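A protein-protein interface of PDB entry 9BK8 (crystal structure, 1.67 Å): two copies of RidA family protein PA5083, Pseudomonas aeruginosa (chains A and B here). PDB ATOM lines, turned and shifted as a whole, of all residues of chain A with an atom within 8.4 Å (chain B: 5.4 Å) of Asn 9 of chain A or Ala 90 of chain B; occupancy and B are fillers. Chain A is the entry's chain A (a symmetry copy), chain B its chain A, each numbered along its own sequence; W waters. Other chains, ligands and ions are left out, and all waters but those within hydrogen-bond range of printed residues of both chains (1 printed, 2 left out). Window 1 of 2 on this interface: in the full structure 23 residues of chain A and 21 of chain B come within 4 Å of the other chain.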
ATOM      1  N   PRO A   3      23.761 -30.646 -24.153  1.00  0.00           N
ATOM      2  CA  PRO A   3      23.491 -29.820 -22.969  1.00  0.00           C
ATOM      3  C   PRO A   3      22.059 -29.993 -22.473  1.00  0.00           C
ATOM      4  O   PRO A   3      21.122 -30.149 -23.261  1.00  0.00           O
ATOM      5  CB  PRO A   3      23.719 -28.389 -23.462  1.00  0.00           C
ATOM      6  CG  PRO A   3      24.378 -28.491 -24.769  1.00  0.00           C
ATOM      7  CD  PRO A   3      24.090 -29.840 -25.341  1.00  0.00           C
ATOM      8  N   THR A   4      21.892 -29.942 -21.153  1.00  0.00           N
ATOM      9  CA  THR A   4      20.580 -29.871 -20.536  1.00  0.00           C
ATOM     10  C   THR A   4      20.482 -28.560 -19.767  1.00  0.00           C
ATOM     11  O   THR A   4      21.494 -27.957 -19.394  1.00  0.00           O
ATOM     12  CB  THR A   4      20.323 -31.059 -19.621  1.00  0.00           C
ATOM     13  OG1 THR A   4      21.286 -31.070 -18.571  1.00  0.00           O
ATOM     14  CG2 THR A   4      20.419 -32.359 -20.426  1.00  0.00           C
ATOM     15  N   ARG A   5      19.256 -28.111 -19.561  1.00  0.00           N
ATOM     16  CA  ARG A   5      19.007 -26.784 -19.021  1.00  0.00           C
ATOM     17  C   ARG A   5      18.076 -26.842 -17.819  1.00  0.00           C
ATOM     18  O   ARG A   5      17.195 -27.701 -17.724  1.00  0.00           O
ATOM     19  CB  ARG A   5      18.421 -25.866 -20.093  1.00  0.00           C
ATOM     20  CG  ARG A   5      19.271 -25.792 -21.352  1.00  0.00           C
ATOM     21  CD  ARG A   5      18.695 -24.858 -22.364  1.00  0.00           C
ATOM     22  NE  ARG A   5      19.516 -24.822 -23.562  1.00  0.00           N
ATOM     23  CZ  ARG A   5      19.499 -25.742 -24.510  1.00  0.00           C
ATOM     24  NH1 ARG A   5      18.691 -26.786 -24.439  1.00  0.00           N
ATOM     25  NH2 ARG A   5      20.310 -25.613 -25.551  1.00  0.00           N
ATOM     26  N   ILE A   6      18.301 -25.917 -16.888  1.00  0.00           N
ATOM     27  CA  ILE A   6      17.472 -25.742 -15.703  1.00  0.00           C
ATOM     28  C   ILE A   6      16.985 -24.297 -15.662  1.00  0.00           C
ATOM     29  O   ILE A   6      17.791 -23.355 -15.720  1.00  0.00           O
ATOM     30  CB  ILE A   6      18.248 -26.093 -14.423  1.00  0.00           C
ATOM     31  CG1 ILE A   6      18.659 -27.568 -14.405  1.00  0.00           C
ATOM     32  CG2 ILE A   6      17.439 -25.732 -13.157  1.00  0.00           C
ATOM     33  CD1 ILE A   6      19.796 -27.864 -13.428  1.00  0.00           C
ATOM     34  N   ALA A   7      15.657 -24.134 -15.568  1.00  0.00           N
ATOM     35  CA  ALA A   7      14.985 -22.847 -15.399  1.00  0.00           C
ATOM     36  C   ALA A   7      15.268 -21.907 -16.578  1.00  0.00           C
ATOM     37  O   ALA A   7      15.923 -20.865 -16.462  1.00  0.00           O
ATOM     38  CB  ALA A   7      15.377 -22.211 -14.061  1.00  0.00           C
ATOM     39  N   THR A   8      14.683 -22.277 -17.708  1.00  0.00           N
ATOM     40  CA  THR A   8      14.871 -21.555 -18.959  1.00  0.00           C
ATOM     41  C   THR A   8      13.779 -20.505 -19.147  1.00  0.00           C
ATOM     42  O   THR A   8      12.591 -20.792 -18.965  1.00  0.00           O
ATOM     43  CB  THR A   8      14.861 -22.538 -20.134  1.00  0.00           C
ATOM     44  OG1 THR A   8      15.887 -23.526 -19.976  1.00  0.00           O
ATOM     45  CG2 THR A   8      15.041 -21.805 -21.446  1.00  0.00           C
ATOM     46  N   ASN A   9      14.187 -19.290 -19.500  1.00  0.00           N
ATOM     47  CA  ASN A   9      13.248 -18.271 -19.943  1.00  0.00           C
ATOM     48  C   ASN A   9      13.702 -17.756 -21.308  1.00  0.00           C
ATOM     49  O   ASN A   9      14.545 -18.378 -21.951  1.00  0.00           O
ATOM     50  CB  ASN A   9      13.102 -17.158 -18.897  1.00  0.00           C
ATOM     51  CG  ASN A   9      14.409 -16.400 -18.621  1.00  0.00           C
ATOM     52  OD1 ASN A   9      15.148 -16.046 -19.528  1.00  0.00           O
ATOM     53  ND2 ASN A   9      14.665 -16.130 -17.354  1.00  0.00           N
ATOM     54  N   ASP A  10      13.140 -16.635 -21.762  1.00  0.00           N
ATOM     55  CA  ASP A  10      13.426 -16.155 -23.108  1.00  0.00           C
ATOM     56  C   ASP A  10      14.844 -15.620 -23.268  1.00  0.00           C
ATOM     57  O   ASP A  10      15.306 -15.467 -24.405  1.00  0.00           O
ATOM     58  CB  ASP A  10      12.448 -15.046 -23.485  1.00  0.00           C
ATOM     59  CG  ASP A  10      11.078 -15.574 -23.858  1.00  0.00           C
ATOM     60  OD1 ASP A  10      10.897 -16.809 -23.839  1.00  0.00           O
ATOM     61  OD2 ASP A  10      10.187 -14.748 -24.172  1.00  0.00           O
ATOM     62  N   ARG A  11      15.532 -15.314 -22.169  1.00  0.00           N
ATOM     63  CA  ARG A  11      16.874 -14.758 -22.242  1.00  0.00           C
ATOM     64  C   ARG A  11      17.973 -15.722 -21.829  1.00  0.00           C
ATOM     65  O   ARG A  11      19.098 -15.599 -22.318  1.00  0.00           O
ATOM     66  CB  ARG A  11      17.000 -13.530 -21.336  1.00  0.00           C
ATOM     67  CG  ARG A  11      16.064 -12.407 -21.653  1.00  0.00           C
ATOM     68  CD  ARG A  11      16.059 -11.420 -20.487  1.00  0.00           C
ATOM     69  NE  ARG A  11      15.108 -10.343 -20.716  1.00  0.00           N
ATOM     70  CZ  ARG A  11      14.925  -9.318 -19.899  1.00  0.00           C
ATOM     71  NH1 ARG A  11      15.629  -9.189 -18.782  1.00  0.00           N
ATOM     72  NH2 ARG A  11      14.012  -8.403 -20.207  1.00  0.00           N
ATOM     73  N   LEU A  12      17.696 -16.619 -20.894  1.00  0.00           N
ATOM     74  CA  LEU A  12      18.739 -17.407 -20.274  1.00  0.00           C
ATOM     75  C   LEU A  12      18.148 -18.642 -19.614  1.00  0.00           C
ATOM     76  O   LEU A  12      16.942 -18.727 -19.350  1.00  0.00           O
ATOM     77  CB  LEU A  12      19.508 -16.569 -19.250  1.00  0.00           C
ATOM     78  CG  LEU A  12      18.703 -15.899 -18.126  1.00  0.00           C
ATOM     79  CD1 LEU A  12      18.473 -16.878 -17.015  1.00  0.00           C
ATOM     80  CD2 LEU A  12      19.445 -14.656 -17.592  1.00  0.00           C
ATOM     81  N   SER A  13      19.034 -19.579 -19.311  1.00  0.00           N
ATOM     82  CA  SER A  13      18.755 -20.658 -18.381  1.00  0.00           C
ATOM     83  C   SER A  13      19.585 -20.446 -17.125  1.00  0.00           C
ATOM     84  O   SER A  13      20.790 -20.146 -17.197  1.00  0.00           O
ATOM     85  CB  SER A  13      19.062 -22.040 -18.976  1.00  0.00           C
ATOM     86  OG  SER A  13      18.311 -22.261 -20.144  1.00  0.00           O
ATOM     87  N   ALA A  14      18.950 -20.645 -15.970  1.00  0.00           N
ATOM     88  CA  ALA A  14      19.665 -20.472 -14.718  1.00  0.00           C
ATOM     89  C   ALA A  14      20.886 -21.369 -14.667  1.00  0.00           C
ATOM     90  O   ALA A  14      21.924 -20.970 -14.130  1.00  0.00           O
ATOM     91  CB  ALA A  14      18.749 -20.753 -13.527  1.00  0.00           C
ATOM     92  N   ALA A  15      20.770 -22.606 -15.176  1.00  0.00           N
ATOM     93  CA  ALA A  15      21.935 -23.473 -15.272  1.00  0.00           C
ATOM     94  C   ALA A  15      21.916 -24.238 -16.588  1.00  0.00           C
ATOM     95  O   ALA A  15      20.852 -24.585 -17.101  1.00  0.00           O
ATOM     96  CB  ALA A  15      22.003 -24.460 -14.110  1.00  0.00           C
ATOM     97  N   VAL A  16      23.098 -24.450 -17.152  1.00  0.00           N
ATOM     98  CA  VAL A  16      23.285 -25.357 -18.282  1.00  0.00           C
ATOM     99  C   VAL A  16      24.305 -26.408 -17.880  1.00  0.00           C
ATOM    100  O   VAL A  16      25.415 -26.083 -17.450  1.00  0.00           O
ATOM    101  CB  VAL A  16      23.730 -24.623 -19.553  1.00  0.00           C
ATOM    102  CG1 VAL A  16      23.994 -25.628 -20.645  1.00  0.00           C
ATOM    103  CG2 VAL A  16      22.666 -23.636 -19.996  1.00  0.00           C
ATOM    104  N   SER A  25      24.069 -19.120 -14.747  1.00  0.00           N
ATOM    105  CA  SER A  25      23.890 -17.706 -15.025  1.00  0.00           C
ATOM    106  C   SER A  25      24.345 -16.883 -13.830  1.00  0.00           C
ATOM    107  O   SER A  25      24.267 -17.311 -12.675  1.00  0.00           O
ATOM    108  CB  SER A  25      22.430 -17.391 -15.341  1.00  0.00           C
ATOM    109  OG  SER A  25      22.047 -17.837 -16.636  1.00  0.00           O
ATOM    110  N   LEU B  85      17.996 -16.185 -30.375  1.00  0.00           N
ATOM    111  CA  LEU B  85      18.175 -17.478 -29.746  1.00  0.00           C
ATOM    112  C   LEU B  85      17.214 -18.528 -30.311  1.00  0.00           C
ATOM    113  O   LEU B  85      16.062 -18.229 -30.633  1.00  0.00           O
ATOM    114  CB  LEU B  85      17.954 -17.385 -28.245  1.00  0.00           C
ATOM    115  CG  LEU B  85      19.060 -16.773 -27.366  1.00  0.00           C
ATOM    116  CD1 LEU B  85      18.549 -16.738 -25.916  1.00  0.00           C
ATOM    117  CD2 LEU B  85      20.340 -17.535 -27.472  1.00  0.00           C
ATOM    118  N   PRO B  86      17.653 -19.778 -30.367  1.00  0.00           N
ATOM    119  CA  PRO B  86      16.705 -20.854 -30.682  1.00  0.00           C
ATOM    120  C   PRO B  86      15.692 -21.031 -29.564  1.00  0.00           C
ATOM    121  O   PRO B  86      16.025 -20.985 -28.378  1.00  0.00           O
ATOM    122  CB  PRO B  86      17.603 -22.089 -30.835  1.00  0.00           C
ATOM    123  CG  PRO B  86      18.858 -21.773 -30.078  1.00  0.00           C
ATOM    124  CD  PRO B  86      18.982 -20.265 -29.972  1.00  0.00           C
ATOM    125  N   GLY B  88      13.328 -21.896 -26.630  1.00  0.00           N
ATOM    126  CA  GLY B  88      13.435 -22.767 -25.482  1.00  0.00           C
ATOM    127  C   GLY B  88      14.829 -23.233 -25.149  1.00  0.00           C
ATOM    128  O   GLY B  88      14.988 -24.088 -24.270  1.00  0.00           O
ATOM    129  N   GLN B  89      15.853 -22.699 -25.809  1.00  0.00           N
ATOM    130  CA  GLN B  89      17.201 -23.231 -25.694  1.00  0.00           C
ATOM    131  C   GLN B  89      18.214 -22.152 -25.331  1.00  0.00           C
ATOM    132  O   GLN B  89      19.346 -22.148 -25.816  1.00  0.00           O
ATOM    133  CB  GLN B  89      17.592 -23.938 -26.983  1.00  0.00           C
ATOM    134  CG  GLN B  89      16.737 -25.198 -27.194  1.00  0.00           C
ATOM    135  CD  GLN B  89      16.771 -25.695 -28.616  1.00  0.00           C
ATOM    136  OE1 GLN B  89      16.060 -25.177 -29.475  1.00  0.00           O
ATOM    137  NE2 GLN B  89      17.589 -26.690 -28.871  1.00  0.00           N
ATOM    138  N   ALA B  90      17.838 -21.249 -24.428  1.00  0.00           N
ATOM    139  CA  ALA B  90      18.757 -20.192 -24.035  1.00  0.00           C
ATOM    140  C   ALA B  90      19.894 -20.738 -23.169  1.00  0.00           C
ATOM    141  O   ALA B  90      19.706 -21.660 -22.369  1.00  0.00           O
ATOM    142  CB  ALA B  90      18.017 -19.100 -23.285  1.00  0.00           C
ATOM    143  N   PRO B  91      21.082 -20.151 -23.291  1.00  0.00           N
ATOM    144  CA  PRO B  91      22.234 -20.592 -22.499  1.00  0.00           C
ATOM    145  C   PRO B  91      22.255 -19.924 -21.121  1.00  0.00           C
ATOM    146  O   PRO B  91      21.443 -19.056 -20.803  1.00  0.00           O
ATOM    147  CB  PRO B  91      23.414 -20.138 -23.374  1.00  0.00           C
ATOM    148  CG  PRO B  91      22.932 -18.819 -23.959  1.00  0.00           C
ATOM    149  CD  PRO B  91      21.438 -19.084 -24.248  1.00  0.00           C
ATOM    150  N   SER B  92      23.237 -20.307 -20.306  1.00  0.00           N
ATOM    151  CA  SER B  92      23.522 -19.484 -19.137  1.00  0.00           C
ATOM    152  C   SER B  92      24.070 -18.135 -19.600  1.00  0.00           C
ATOM    153  O   SER B  92      24.701 -18.025 -20.653  1.00  0.00           O
ATOM    154  CB  SER B  92      24.498 -20.178 -18.176  1.00  0.00           C
ATOM    155  OG  SER B  92      25.813 -20.290 -18.659  1.00  0.00           O
HETATM  156  O   HOH W   1      21.919 -23.398 -24.579  1.00  0.00           O
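The backbone carbonyl oxygen (O) of Ala 90 of chain B sits close to the guanidinium group (NE) of Arg 5 of chain A (3.4 Å). O of Ala 90 of chain B is in hydrogen-bond range of OG of Ser 13 of chain A (2.7 Å). O of Pro 91 of chain B lies within hydrogen-bond range of N of Ser 13 of chain A, at 2.9 Å.
The side-chain hydroxyl of Thr 8 of chain A lies within hydrogen-bond range of the side-chain hydroxyl of Ser 13 of chain A (2.7 Å). The backbone NH (N) of Arg 11 of chain A sits at hydrogen-bond distance from the side-chain amide oxygen (OD1) of Asn 9 of chain A, at 2.8 Å. The side-chain amide oxygen (OD1) of Asn 9 of chain A sits at hydrogen-bond distance from the backbone NH (N) of Leu 12 of chain A, at 2.9 Å. The backbone carbonyl oxygen (O) of Ser 13 of chain A lies within hydrogen-bond range of the side-chain hydroxyl (OG) of Ser 25 of chain A, at 2.7 Å. N of Ser 25 of chain A is in hydrogen-bond range of O of Ala 14 of chain A, at 2.9 Å.
Among the printed residues, pairs that only touch across the chains: Arg 5 of chain A with Gln 89 of chain B (3.5 Å), Thr 8 of chain A with Gly 88 of chain B (3.6 Å), Asn 9 of chain A with Ala 90 of chain B (3.8 Å), Asp 10 of chain A with Leu 85 of chain B (3.8 Å), Arg 11 of chain A with Leu 85 of chain B (3.8 Å), Arg 11 of chain A with Ala 90 of chain B (3.7 Å), Leu 12 of chain A with Ala 90 of chain B (3.5 Å), Leu 12 of chain A with Pro 91 of chain B (3.2 Å), Ser 13 of chain A with Ser 92 of chain B (3.4 Å), Val 16 of chain A with Pro 91 of chain B (3.9 Å), Val 16 of chain A with Ser 92 of chain B (3.4 Å) and Ser 25 of chain A with Ser 92 of chain B (3.3 Å).
Of chain B, only Ala 90 comes within 4 Å of Asn 9 of chain A. Of the printed residues of chain A, Pro 91 of chain B touches Leu 12 (3.2 Å), Ser 13 (2.9 Å) and Val 16 (3.9 Å). Of the printed residues of chain B, Arg 5 of chain A touches Gln 89 (3.5 Å) and Ala 90 (3.4 Å). Of the printed residues of chain B, Asp 10 of chain A touches Leu 85. Printed residues of chain B within 4 Å of Val 16 of chain A: Pro 91 (3.9 Å) and Ser 92 (3.4 Å). Ala 7 of chain A touches none of the printed residues of chain B. Ala 14 of chain A touches none of the printed residues of chain B. The nearest printed residue of chain B that does not touch Asn 9 of chain A is Gly 88 of chain B (5.7 Å). The nearest residue of chain A that does not touch Ala 90 of chain B is Thr 8 of chain A (4.1 Å). The nearest printed residue of chain B that does not touch Ser 13 of chain A is Gln 89 of chain B (5.2 Å).
Of the 15 printed residues of chain A, 9 touch a printed residue of chain B. Hydrophobic or aromatic side chains of chain A that line the printed part of chain B: Leu 12 and Val 16. Among the printed residues, no Asp or Glu carboxylate lies within 4 Å of a Lys or Arg side-chain nitrogen of the other chain.
No position is printed for both chains. Of the 15 pairs that touch across the chains among the printed residues, none has its exchanged pair printed and touching as well.
Water W1 bridges the guanidinium group (NH2) of Arg 5 of chain A (2.9 Å) and the backbone carbonyl oxygen (O) of Gln 89 of chain B (3.1 Å).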
